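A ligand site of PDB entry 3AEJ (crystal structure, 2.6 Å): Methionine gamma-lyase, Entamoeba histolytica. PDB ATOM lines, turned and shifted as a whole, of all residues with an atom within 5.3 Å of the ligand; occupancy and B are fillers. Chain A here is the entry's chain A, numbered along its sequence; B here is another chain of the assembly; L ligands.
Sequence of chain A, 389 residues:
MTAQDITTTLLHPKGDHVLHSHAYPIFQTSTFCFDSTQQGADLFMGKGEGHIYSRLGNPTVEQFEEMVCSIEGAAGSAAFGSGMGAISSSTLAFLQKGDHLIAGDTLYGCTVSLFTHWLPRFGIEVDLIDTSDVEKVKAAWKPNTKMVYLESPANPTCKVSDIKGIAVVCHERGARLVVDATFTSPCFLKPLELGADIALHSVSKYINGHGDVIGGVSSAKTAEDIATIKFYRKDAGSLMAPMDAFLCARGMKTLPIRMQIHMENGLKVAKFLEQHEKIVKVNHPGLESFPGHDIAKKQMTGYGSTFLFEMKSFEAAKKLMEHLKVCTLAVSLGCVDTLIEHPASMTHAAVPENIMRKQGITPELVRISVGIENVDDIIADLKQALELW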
ATOM      1  N   SER A  82     -14.085 -11.377 -14.683  1.00  0.00           N
ATOM      2  CA  SER A  82     -13.176 -12.516 -14.700  1.00  0.00           C
ATOM      3  C   SER A  82     -11.745 -12.009 -14.897  1.00  0.00           C
ATOM      4  O   SER A  82     -11.540 -10.863 -15.303  1.00  0.00           O
ATOM      5  CB  SER A  82     -13.537 -13.488 -15.829  1.00  0.00           C
ATOM      6  OG  SER A  82     -13.207 -12.936 -17.094  1.00  0.00           O
ATOM      7  N   GLY A  83     -10.780 -12.890 -14.608  1.00  0.00           N
ATOM      8  CA  GLY A  83      -9.378 -12.621 -14.910  1.00  0.00           C
ATOM      9  C   GLY A  83      -9.174 -12.393 -16.392  1.00  0.00           C
ATOM     10  O   GLY A  83      -8.397 -11.535 -16.803  1.00  0.00           O
ATOM     11  N   MET A  84      -9.901 -13.163 -17.191  1.00  0.00           N
ATOM     12  CA  MET A  84      -9.885 -13.008 -18.644  1.00  0.00           C
ATOM     13  C   MET A  84     -10.477 -11.673 -19.087  1.00  0.00           C
ATOM     14  O   MET A  84     -10.134 -11.150 -20.144  1.00  0.00           O
ATOM     15  CB  MET A  84     -10.612 -14.171 -19.328  1.00  0.00           C
ATOM     16  CG  MET A  84      -9.904 -15.529 -19.192  1.00  0.00           C
ATOM     17  SD  MET A  84      -8.121 -15.478 -19.544  1.00  0.00           S
ATOM     18  CE  MET A  84      -8.095 -14.936 -21.248  1.00  0.00           C
ATOM     19  N   GLY A  85     -11.379 -11.120 -18.260  1.00  0.00           N
ATOM     20  CA  GLY A  85     -11.879  -9.774 -18.453  1.00  0.00           C
ATOM     21  C   GLY A  85     -10.776  -8.763 -18.232  1.00  0.00           C
ATOM     22  O   GLY A  85     -10.657  -7.783 -18.981  1.00  0.00           O
ATOM     23  N   ILE A  87      -7.446  -9.489 -18.437  1.00  0.00           N
ATOM     24  CA  ILE A  87      -6.389  -9.732 -19.427  1.00  0.00           C
ATOM     25  C   ILE A  87      -6.711  -9.055 -20.773  1.00  0.00           C
ATOM     26  O   ILE A  87      -5.839  -8.390 -21.357  1.00  0.00           O
ATOM     27  CB  ILE A  87      -6.109 -11.245 -19.608  1.00  0.00           C
ATOM     28  CG1 ILE A  87      -5.527 -11.808 -18.304  1.00  0.00           C
ATOM     29  CG2 ILE A  87      -5.139 -11.483 -20.761  1.00  0.00           C
ATOM     30  CD1 ILE A  87      -5.581 -13.325 -18.184  1.00  0.00           C
ATOM     31  N   TYR A 108      -1.325 -19.205 -19.047  1.00  0.00           N
ATOM     32  CA  TYR A 108      -2.606 -19.861 -18.754  1.00  0.00           C
ATOM     33  C   TYR A 108      -3.334 -20.204 -20.058  1.00  0.00           C
ATOM     34  O   TYR A 108      -3.270 -19.442 -21.031  1.00  0.00           O
ATOM     35  CB  TYR A 108      -3.474 -18.993 -17.846  1.00  0.00           C
ATOM     36  CG  TYR A 108      -4.922 -19.436 -17.792  1.00  0.00           C
ATOM     37  CD1 TYR A 108      -5.268 -20.697 -17.312  1.00  0.00           C
ATOM     38  CD2 TYR A 108      -5.943 -18.587 -18.231  1.00  0.00           C
ATOM     39  CE1 TYR A 108      -6.593 -21.122 -17.289  1.00  0.00           C
ATOM     40  CE2 TYR A 108      -7.269 -18.994 -18.201  1.00  0.00           C
ATOM     41  CZ  TYR A 108      -7.592 -20.255 -17.719  1.00  0.00           C
ATOM     42  OH  TYR A 108      -8.896 -20.662 -17.688  1.00  0.00           O
ATOM     43  N   CYS A 110      -6.392 -20.164 -21.423  1.00  0.00           N
ATOM     44  CA  CYS A 110      -7.290 -19.240 -22.118  1.00  0.00           C
ATOM     45  C   CYS A 110      -6.603 -17.940 -22.538  1.00  0.00           C
ATOM     46  O   CYS A 110      -7.059 -17.261 -23.461  1.00  0.00           O
ATOM     47  CB  CYS A 110      -8.551 -18.960 -21.295  1.00  0.00           C
ATOM     48  SG  CYS A 110      -9.580 -20.429 -21.009  1.00  0.00           S
ATOM     49  N   THR A 111      -5.499 -17.596 -21.864  1.00  0.00           N
ATOM     50  CA  THR A 111      -4.657 -16.481 -22.279  1.00  0.00           C
ATOM     51  C   THR A 111      -4.000 -16.811 -23.613  1.00  0.00           C
ATOM     52  O   THR A 111      -3.914 -15.954 -24.503  1.00  0.00           O
ATOM     53  CB  THR A 111      -3.587 -16.127 -21.217  1.00  0.00           C
ATOM     54  OG1 THR A 111      -4.213 -15.957 -19.939  1.00  0.00           O
ATOM     55  CG2 THR A 111      -2.862 -14.840 -21.583  1.00  0.00           C
ATOM     56  N   GLU A 151       3.846 -13.915 -17.494  1.00  0.00           N
ATOM     57  CA  GLU A 151       3.353 -14.643 -16.335  1.00  0.00           C
ATOM     58  C   GLU A 151       4.569 -15.218 -15.612  1.00  0.00           C
ATOM     59  O   GLU A 151       5.355 -15.952 -16.216  1.00  0.00           O
ATOM     60  CB  GLU A 151       2.435 -15.791 -16.749  1.00  0.00           C
ATOM     61  CG  GLU A 151       0.974 -15.413 -16.907  1.00  0.00           C
ATOM     62  CD  GLU A 151       0.075 -16.622 -17.137  1.00  0.00           C
ATOM     63  OE1 GLU A 151       0.227 -17.636 -16.417  1.00  0.00           O
ATOM     64  OE2 GLU A 151      -0.786 -16.558 -18.039  1.00  0.00           O
ATOM     65  N   ASN A 155       1.870 -20.376 -15.252  1.00  0.00           N
ATOM     66  CA  ASN A 155       0.873 -21.435 -15.117  1.00  0.00           C
ATOM     67  C   ASN A 155       1.068 -22.440 -16.254  1.00  0.00           C
ATOM     68  O   ASN A 155       0.975 -22.055 -17.425  1.00  0.00           O
ATOM     69  CB  ASN A 155      -0.533 -20.824 -15.157  1.00  0.00           C
ATOM     70  CG  ASN A 155      -1.623 -21.796 -14.735  1.00  0.00           C
ATOM     71  OD1 ASN A 155      -1.405 -22.992 -14.578  1.00  0.00           O
ATOM     72  ND2 ASN A 155      -2.824 -21.263 -14.538  1.00  0.00           N
ATOM     73  N   ASP A 180       1.001 -10.705 -15.296  1.00  0.00           N
ATOM     74  CA  ASP A 180      -0.054 -11.447 -14.606  1.00  0.00           C
ATOM     75  C   ASP A 180       0.568 -12.089 -13.366  1.00  0.00           C
ATOM     76  O   ASP A 180       1.424 -12.971 -13.469  1.00  0.00           O
ATOM     77  CB  ASP A 180      -0.651 -12.508 -15.529  1.00  0.00           C
ATOM     78  CG  ASP A 180      -1.868 -13.212 -14.931  1.00  0.00           C
ATOM     79  OD1 ASP A 180      -1.986 -13.312 -13.703  1.00  0.00           O
ATOM     80  OD2 ASP A 180      -2.719 -13.680 -15.727  1.00  0.00           O
ATOM     81  N   THR A 182      -1.193 -13.528 -10.749  1.00  0.00           N
ATOM     82  CA  THR A 182      -2.205 -14.364 -10.090  1.00  0.00           C
ATOM     83  C   THR A 182      -1.604 -15.448  -9.184  1.00  0.00           C
ATOM     84  O   THR A 182      -2.054 -15.624  -8.052  1.00  0.00           O
ATOM     85  CB  THR A 182      -3.146 -15.025 -11.144  1.00  0.00           C
ATOM     86  OG1 THR A 182      -3.773 -14.015 -11.937  1.00  0.00           O
ATOM     87  CG2 THR A 182      -4.217 -15.881 -10.467  1.00  0.00           C
ATOM     88  N   PHE A 183      -0.585 -16.141  -9.692  1.00  0.00           N
ATOM     89  CA  PHE A 183       0.048 -17.270  -9.002  1.00  0.00           C
ATOM     90  C   PHE A 183       0.712 -16.933  -7.664  1.00  0.00           C
ATOM     91  O   PHE A 183       0.882 -17.807  -6.816  1.00  0.00           O
ATOM     92  CB  PHE A 183       1.084 -17.933  -9.913  1.00  0.00           C
ATOM     93  CG  PHE A 183       0.687 -19.294 -10.404  1.00  0.00           C
ATOM     94  CD1 PHE A 183      -0.562 -19.525 -10.974  1.00  0.00           C
ATOM     95  CD2 PHE A 183       1.587 -20.355 -10.327  1.00  0.00           C
ATOM     96  CE1 PHE A 183      -0.917 -20.785 -11.442  1.00  0.00           C
ATOM     97  CE2 PHE A 183       1.236 -21.621 -10.783  1.00  0.00           C
ATOM     98  CZ  PHE A 183      -0.013 -21.842 -11.349  1.00  0.00           C
ATOM     99  N   SER A 202      -6.196 -12.648 -11.652  1.00  0.00           N
ATOM    100  CA  SER A 202      -7.455 -13.338 -11.551  1.00  0.00           C
ATOM    101  C   SER A 202      -7.800 -13.361 -10.070  1.00  0.00           C
ATOM    102  O   SER A 202      -7.193 -14.103  -9.289  1.00  0.00           O
ATOM    103  CB  SER A 202      -7.351 -14.761 -12.111  1.00  0.00           C
ATOM    104  OG  SER A 202      -8.555 -15.467 -11.921  1.00  0.00           O
ATOM    105  N   VAL A 203      -8.735 -12.490  -9.680  1.00  0.00           N
ATOM    106  CA  VAL A 203      -9.199 -12.394  -8.302  1.00  0.00           C
ATOM    107  C   VAL A 203      -9.873 -13.701  -7.864  1.00  0.00           C
ATOM    108  O   VAL A 203      -9.934 -14.011  -6.676  1.00  0.00           O
ATOM    109  CB  VAL A 203     -10.174 -11.212  -8.116  1.00  0.00           C
ATOM    110  CG1 VAL A 203     -10.579 -11.065  -6.653  1.00  0.00           C
ATOM    111  CG2 VAL A 203      -9.546  -9.937  -8.608  1.00  0.00           C
ATOM    112  N   SER A 204     -10.355 -14.455  -8.850  1.00  0.00           N
ATOM    113  CA  SER A 204     -10.958 -15.773  -8.626  1.00  0.00           C
ATOM    114  C   SER A 204     -10.088 -16.698  -7.785  1.00  0.00           C
ATOM    115  O   SER A 204     -10.583 -17.637  -7.154  1.00  0.00           O
ATOM    116  CB  SER A 204     -11.251 -16.435  -9.971  1.00  0.00           C
ATOM    117  OG  SER A 204     -11.736 -15.505 -10.917  1.00  0.00           O
ATOM    118  N   LYS A 205      -8.775 -16.431  -7.776  1.00  0.00           N
ATOM    119  CA  LYS A 205      -7.828 -17.287  -7.083  1.00  0.00           C
ATOM    120  C   LYS A 205      -7.496 -16.819  -5.669  1.00  0.00           C
ATOM    121  O   LYS A 205      -8.379 -16.831  -4.808  1.00  0.00           O
ATOM    122  CB  LYS A 205      -6.571 -17.506  -7.942  1.00  0.00           C
ATOM    123  CG  LYS A 205      -6.763 -18.556  -9.031  1.00  0.00           C
ATOM    124  CD  LYS A 205      -7.346 -17.975 -10.303  1.00  0.00           C
ATOM    125  CE  LYS A 205      -8.557 -18.752 -10.780  1.00  0.00           C
ATOM    126  NZ  LYS A 205      -8.259 -20.181 -11.074  1.00  0.00           N
ATOM    127  N   ILE A 214     -15.852 -15.617  -9.378  1.00  0.00           N
ATOM    128  CA  ILE A 214     -15.020 -15.409 -10.555  1.00  0.00           C
ATOM    129  C   ILE A 214     -14.826 -13.905 -10.709  1.00  0.00           C
ATOM    130  O   ILE A 214     -15.802 -13.157 -10.804  1.00  0.00           O
ATOM    131  CB  ILE A 214     -15.670 -15.963 -11.849  1.00  0.00           C
ATOM    132  CG1 ILE A 214     -16.149 -17.409 -11.673  1.00  0.00           C
ATOM    133  CG2 ILE A 214     -14.730 -15.794 -13.054  1.00  0.00           C
ATOM    134  CD1 ILE A 214     -15.064 -18.467 -11.735  1.00  0.00           C
ATOM    135  N   GLY A 215     -13.576 -13.470 -10.735  1.00  0.00           N
ATOM    136  CA  GLY A 215     -13.270 -12.047 -10.848  1.00  0.00           C
ATOM    137  C   GLY A 215     -11.875 -11.734 -11.322  1.00  0.00           C
ATOM    138  O   GLY A 215     -10.973 -12.573 -11.251  1.00  0.00           O
ATOM    139  N   GLY A 216     -11.694 -10.500 -11.801  1.00  0.00           N
ATOM    140  CA  GLY A 216     -10.395 -10.028 -12.270  1.00  0.00           C
ATOM    141  C   GLY A 216     -10.130  -8.595 -11.849  1.00  0.00           C
ATOM    142  O   GLY A 216     -11.062  -7.819 -11.615  1.00  0.00           O
ATOM    143  N   VAL A 331     -10.259 -28.134 -11.212  1.00  0.00           N
ATOM    144  CA  VAL A 331      -9.442 -27.053 -11.771  1.00  0.00           C
ATOM    145  C   VAL A 331      -9.517 -25.817 -10.868  1.00  0.00           C
ATOM    146  O   VAL A 331     -10.175 -25.838  -9.825  1.00  0.00           O
ATOM    147  CB  VAL A 331      -9.808 -26.702 -13.247  1.00  0.00           C
ATOM    148  CG1 VAL A 331      -9.598 -27.909 -14.157  1.00  0.00           C
ATOM    149  CG2 VAL A 331     -11.237 -26.167 -13.363  1.00  0.00           C
ATOM    150  N   SER A 332      -8.840 -24.747 -11.290  1.00  0.00           N
ATOM    151  CA  SER A 332      -8.670 -23.521 -10.495  1.00  0.00           C
ATOM    152  C   SER A 332      -7.627 -23.704  -9.389  1.00  0.00           C
ATOM    153  O   SER A 332      -7.112 -24.808  -9.198  1.00  0.00           O
ATOM    154  CB  SER A 332     -10.002 -23.005  -9.932  1.00  0.00           C
ATOM    155  OG  SER A 332      -9.837 -21.734  -9.333  1.00  0.00           O
ATOM    156  N   LEU A 333      -7.311 -22.627  -8.691  1.00  0.00           N
ATOM    157  CA  LEU A 333      -6.277 -22.635  -7.658  1.00  0.00           C
ATOM    158  C   LEU A 333      -6.472 -21.505  -6.650  1.00  0.00           C
ATOM    159  O   LEU A 333      -7.445 -20.744  -6.724  1.00  0.00           O
ATOM    160  CB  LEU A 333      -4.886 -22.505  -8.284  1.00  0.00           C
ATOM    161  CG  LEU A 333      -4.675 -21.325  -9.248  1.00  0.00           C
ATOM    162  CD1 LEU A 333      -3.439 -20.520  -8.856  1.00  0.00           C
ATOM    163  CD2 LEU A 333      -4.626 -21.779 -10.692  1.00  0.00           C
ATOM    164  N   GLU A 341      -5.116 -31.047 -10.077  1.00  0.00           N
ATOM    165  CA  GLU A 341      -5.561 -31.248 -11.458  1.00  0.00           C
ATOM    166  C   GLU A 341      -4.472 -31.785 -12.379  1.00  0.00           C
ATOM    167  O   GLU A 341      -3.292 -31.829 -12.006  1.00  0.00           O
ATOM    168  CB  GLU A 341      -6.192 -29.958 -12.021  1.00  0.00           C
ATOM    169  CG  GLU A 341      -5.226 -28.787 -12.210  1.00  0.00           C
ATOM    170  CD  GLU A 341      -4.822 -28.566 -13.662  1.00  0.00           C
ATOM    171  OE1 GLU A 341      -4.029 -27.635 -13.917  1.00  0.00           O
ATOM    172  OE2 GLU A 341      -5.303 -29.300 -14.549  1.00  0.00           O
ATOM    173  N   MET A 346      -6.640 -31.243 -18.762  1.00  0.00           N
ATOM    174  CA  MET A 346      -7.594 -30.299 -18.172  1.00  0.00           C
ATOM    175  C   MET A 346      -7.317 -28.834 -18.547  1.00  0.00           C
ATOM    176  O   MET A 346      -7.761 -28.379 -19.606  1.00  0.00           O
ATOM    177  CB  MET A 346      -7.697 -30.496 -16.653  1.00  0.00           C
ATOM    178  CG  MET A 346      -8.303 -31.839 -16.254  1.00  0.00           C
ATOM    179  SD  MET A 346      -8.100 -32.262 -14.507  1.00  0.00           S
ATOM    180  CE  MET A 346      -8.875 -33.876 -14.464  1.00  0.00           C
ATOM    181  N   THR A 347      -6.588 -28.107 -17.703  1.00  0.00           N
ATOM    182  CA  THR A 347      -6.360 -26.668 -17.881  1.00  0.00           C
ATOM    183  C   THR A 347      -5.616 -26.287 -19.154  1.00  0.00           C
ATOM    184  O   THR A 347      -5.798 -25.184 -19.686  1.00  0.00           O
ATOM    185  CB  THR A 347      -5.631 -26.033 -16.665  1.00  0.00           C
ATOM    186  OG1 THR A 347      -4.445 -26.783 -16.357  1.00  0.00           O
ATOM    187  CG2 THR A 347      -6.539 -25.999 -15.445  1.00  0.00           C
ATOM    188  N   HIS A 348      -4.774 -27.202 -19.647  1.00  0.00           N
ATOM    189  CA  HIS A 348      -3.982 -26.954 -20.841  1.00  0.00           C
ATOM    190  C   HIS A 348      -4.188 -28.052 -21.899  1.00  0.00           C
ATOM    191  O   HIS A 348      -3.237 -28.484 -22.551  1.00  0.00           O
ATOM    192  CB  HIS A 348      -2.504 -26.805 -20.487  1.00  0.00           C
ATOM    193  CG  HIS A 348      -2.217 -25.671 -19.552  1.00  0.00           C
ATOM    194  ND1 HIS A 348      -1.797 -24.429 -19.985  1.00  0.00           N
ATOM    195  CD2 HIS A 348      -2.294 -25.584 -18.199  1.00  0.00           C
ATOM    196  CE1 HIS A 348      -1.632 -23.633 -18.943  1.00  0.00           C
ATOM    197  NE2 HIS A 348      -1.930 -24.311 -17.857  1.00  0.00           N
ATOM    198  N   ARG A 367      -0.553 -30.798 -11.233  1.00  0.00           N
ATOM    199  CA  ARG A 367      -0.511 -29.490 -10.578  1.00  0.00           C
ATOM    200  C   ARG A 367      -1.301 -29.512  -9.276  1.00  0.00           C
ATOM    201  O   ARG A 367      -2.457 -29.915  -9.242  1.00  0.00           O
ATOM    202  CB  ARG A 367      -1.031 -28.376 -11.496  1.00  0.00           C
ATOM    203  CG  ARG A 367      -0.684 -26.974 -11.003  1.00  0.00           C
ATOM    204  CD  ARG A 367      -1.438 -25.903 -11.769  1.00  0.00           C
ATOM    205  NE  ARG A 367      -2.850 -25.875 -11.420  1.00  0.00           N
ATOM    206  CZ  ARG A 367      -3.771 -25.161 -12.064  1.00  0.00           C
ATOM    207  NH1 ARG A 367      -3.435 -24.404 -13.104  1.00  0.00           N
ATOM    208  NH2 ARG A 367      -5.040 -25.215 -11.670  1.00  0.00           N
ATOM    209  N   PHE B  44     -13.853 -31.419 -20.661  1.00  0.00           N
ATOM    210  CA  PHE B  44     -13.022 -30.479 -21.417  1.00  0.00           C
ATOM    211  C   PHE B  44     -13.062 -30.733 -22.919  1.00  0.00           C
ATOM    212  O   PHE B  44     -12.774 -29.834 -23.719  1.00  0.00           O
ATOM    213  CB  PHE B  44     -11.579 -30.521 -20.910  1.00  0.00           C
ATOM    214  CG  PHE B  44     -11.289 -29.545 -19.796  1.00  0.00           C
ATOM    215  CD1 PHE B  44     -11.278 -29.967 -18.478  1.00  0.00           C
ATOM    216  CD2 PHE B  44     -11.024 -28.208 -20.088  1.00  0.00           C
ATOM    217  CE1 PHE B  44     -11.006 -29.063 -17.448  1.00  0.00           C
ATOM    218  CE2 PHE B  44     -10.756 -27.299 -19.069  1.00  0.00           C
ATOM    219  CZ  PHE B  44     -10.740 -27.735 -17.743  1.00  0.00           C
ATOM    220  N   TYR B  53     -16.063 -25.130 -14.576  1.00  0.00           N
ATOM    221  CA  TYR B  53     -15.658 -23.826 -14.057  1.00  0.00           C
ATOM    222  C   TYR B  53     -16.721 -22.820 -14.484  1.00  0.00           C
ATOM    223  O   TYR B  53     -17.236 -22.896 -15.610  1.00  0.00           O
ATOM    224  CB  TYR B  53     -14.299 -23.454 -14.638  1.00  0.00           C
ATOM    225  CG  TYR B  53     -13.619 -22.259 -14.005  1.00  0.00           C
ATOM    226  CD1 TYR B  53     -13.078 -22.331 -12.720  1.00  0.00           C
ATOM    227  CD2 TYR B  53     -13.469 -21.067 -14.711  1.00  0.00           C
ATOM    228  CE1 TYR B  53     -12.435 -21.242 -12.146  1.00  0.00           C
ATOM    229  CE2 TYR B  53     -12.830 -19.972 -14.150  1.00  0.00           C
ATOM    230  CZ  TYR B  53     -12.315 -20.066 -12.866  1.00  0.00           C
ATOM    231  OH  TYR B  53     -11.690 -18.973 -12.301  1.00  0.00           O
ATOM    232  N   ARG B  55     -16.907 -19.769 -15.483  1.00  0.00           N
ATOM    233  CA  ARG B  55     -16.710 -19.015 -16.721  1.00  0.00           C
ATOM    234  C   ARG B  55     -17.127 -19.833 -17.949  1.00  0.00           C
ATOM    235  O   ARG B  55     -17.724 -19.291 -18.895  1.00  0.00           O
ATOM    236  CB  ARG B  55     -15.260 -18.535 -16.856  1.00  0.00           C
ATOM    237  CG  ARG B  55     -14.953 -17.801 -18.163  1.00  0.00           C
ATOM    238  CD  ARG B  55     -13.719 -16.886 -18.059  1.00  0.00           C
ATOM    239  NE  ARG B  55     -12.599 -17.525 -17.374  1.00  0.00           N
ATOM    240  CZ  ARG B  55     -11.769 -18.405 -17.920  1.00  0.00           C
ATOM    241  NH1 ARG B  55     -11.912 -18.792 -19.183  1.00  0.00           N
ATOM    242  NH2 ARG B  55     -10.782 -18.923 -17.194  1.00  0.00           N
ATOM    243  N   LEU B  56     -16.822 -21.126 -17.936  1.00  0.00           N
ATOM    244  CA  LEU B  56     -17.253 -22.044 -18.993  1.00  0.00           C
ATOM    245  C   LEU B  56     -18.745 -22.347 -18.887  1.00  0.00           C
ATOM    246  O   LEU B  56     -19.411 -22.592 -19.894  1.00  0.00           O
ATOM    247  CB  LEU B  56     -16.443 -23.347 -18.946  1.00  0.00           C
ATOM    248  CG  LEU B  56     -14.919 -23.277 -19.117  1.00  0.00           C
ATOM    249  CD1 LEU B  56     -14.309 -24.658 -18.887  1.00  0.00           C
ATOM    250  CD2 LEU B  56     -14.518 -22.742 -20.486  1.00  0.00           C
HETATM  251  N1  LIG L   1      -6.992 -20.476 -14.430  1.00  0.00           N
HETATM  252  C1  LIG L   1      -7.636 -21.632 -13.815  1.00  0.00           C
HETATM  253  C2  LIG L   1      -6.672 -22.787 -13.744  1.00  0.00           C
HETATM  254  O1  LIG L   1      -6.866 -23.700 -12.932  1.00  0.00           O
HETATM  255  C3  LIG L   1      -8.914 -21.904 -14.635  1.00  0.00           C
HETATM  256  C4  LIG L   1      -9.063 -23.334 -15.149  1.00  0.00           C
HETATM  257  S1  LIG L   1     -10.200 -23.393 -16.501  1.00  0.00           S
HETATM  258  C5  LIG L   1      -9.063 -24.054 -17.678  1.00  0.00           C
HETATM  259  O2  LIG L   1      -5.668 -22.800 -14.493  1.00  0.00           O
HETATM  260  C6  LIG L   1      -3.913 -16.941 -14.649  1.00  0.00           C
HETATM  261  C7  LIG L   1      -2.433 -16.758 -14.442  1.00  0.00           C
HETATM  262  C8  LIG L   1      -4.608 -18.132 -14.081  1.00  0.00           C
HETATM  263  C9  LIG L   1      -6.069 -18.254 -14.324  1.00  0.00           C
HETATM  264  C10 LIG L   1      -6.756 -19.438 -13.748  1.00  0.00           C
HETATM  265  C11 LIG L   1      -6.699 -17.244 -15.044  1.00  0.00           C
HETATM  266  C12 LIG L   1      -8.182 -17.303 -15.332  1.00  0.00           C
HETATM  267  C13 LIG L   1      -5.961 -16.163 -15.537  1.00  0.00           C
HETATM  268  N2  LIG L   1      -4.633 -16.033 -15.344  1.00  0.00           N
HETATM  269  O3  LIG L   1     -10.788 -17.704 -14.457  1.00  0.00           O
HETATM  270  O4  LIG L   1     -10.940 -15.672 -15.968  1.00  0.00           O
HETATM  271  O5  LIG L   1      -3.938 -19.081 -13.372  1.00  0.00           O
HETATM  272  O6  LIG L   1     -10.792 -15.381 -13.451  1.00  0.00           O
HETATM  273  O7  LIG L   1      -8.868 -16.200 -14.758  1.00  0.00           O
HETATM  274  P1  LIG L   1     -10.471 -16.236 -14.643  1.00  0.00           P
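The side-chain hydroxyl (OG) of Ser 82 sits at hydrogen-bond distance from the backbone NH (N) of Gly 85 (2.8 Å). The guanidinium group of Arg 367 sits at hydrogen-bond distance from the side-chain amide oxygen of Asn 155, at 2.9 Å. The guanidinium group (NH2) of Arg 367 lies within hydrogen-bond range of the backbone carbonyl oxygen (O) of Ser 332, at 3.3 Å. N of Tyr 108 sits at hydrogen-bond distance from OE2 of Glu 151, at 2.9 Å. The backbone carbonyl oxygen of Gly 215 is in hydrogen-bond range of the backbone NH of Val 203 (2.7 Å). NE of Arg 367 is in salt-bridge range of OE1 of Glu 341, 3.3 Å away. The side-chain hydroxyl (OG) of Ser 204 sits at hydrogen-bond distance from the backbone NH (N) of Gly 215 (2.7 Å). N of Ser 202 is in hydrogen-bond range of OG1 of Thr 182.
OG of Ser 204 is in hydrogen-bond range of O6 of the ligand (2.7 Å). The backbone NH of Gly 83 is in hydrogen-bond range of an oxygen (O6) of the ligand (2.7 Å). O6 of the ligand sits at hydrogen-bond distance from OG of Ser 202 (2.7 Å). The side-chain amide nitrogen of Asn 155 is in hydrogen-bond range of an oxygen (O5) of the ligand. O4 of the ligand is in salt-bridge range of NE of Arg 55 of chain B, 2.9 Å away. An oxygen (O4) of the ligand is in hydrogen-bond range of the backbone NH (N) of Met 84, 3.0 Å away. An oxygen (O1) of the ligand sits at hydrogen-bond distance from the backbone NH (N) of Ser 332, 2.8 Å away. The guanidinium group (NH2) of Arg 367 lies within salt-bridge range of an oxygen (O1) of the ligand (2.7 Å). The side-chain hydroxyl (OH) of Tyr 53 of chain B sits at hydrogen-bond distance from an oxygen (O3) of the ligand (2.7 Å). A sulfur (S1) of the ligand lies close to the side-chain hydroxyl of Tyr 108, at 3.3 Å.
OD2 of Asp 180 lies close to N2 of the ligand, at 3.1 Å. Ser 82 touches the ligand (CB to O4, 3.4 Å). Ile 87 touches the ligand. OE1 of Glu 151 touches C7 of the ligand, at 3.4 Å. Thr 182 touches the ligand (CB to C7, 3.8 Å). Phe 183 touches the ligand (CE1 to O5, 3.97 Å). Lys 205 touches the ligand. CG2 of Ile 214 touches O6 of the ligand, at 3.98 Å. Gly 215 touches the ligand (O to O6, 3.6 Å). CB of Val 331 touches C4 of the ligand (3.9 Å). Leu 333 touches the ligand. Thr 347 touches the ligand (CG2 to O1, 3.4 Å). CE2 of Phe 44 of chain B touches C5 of the ligand, 3.9 Å away. Within 4 Å of the ligand: Ser 82, Gly 83, Met 84, Ile 87, Tyr 108, Glu 151, Asn 155, Asp 180, Thr 182, Phe 183, Ser 202, Ser 204, Lys 205, Ile 214, Gly 215, Val 331, Ser 332, Leu 333, Thr 347, Arg 367, Phe 44 of chain B, Tyr 53 of chain B and Arg 55 of chain B.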
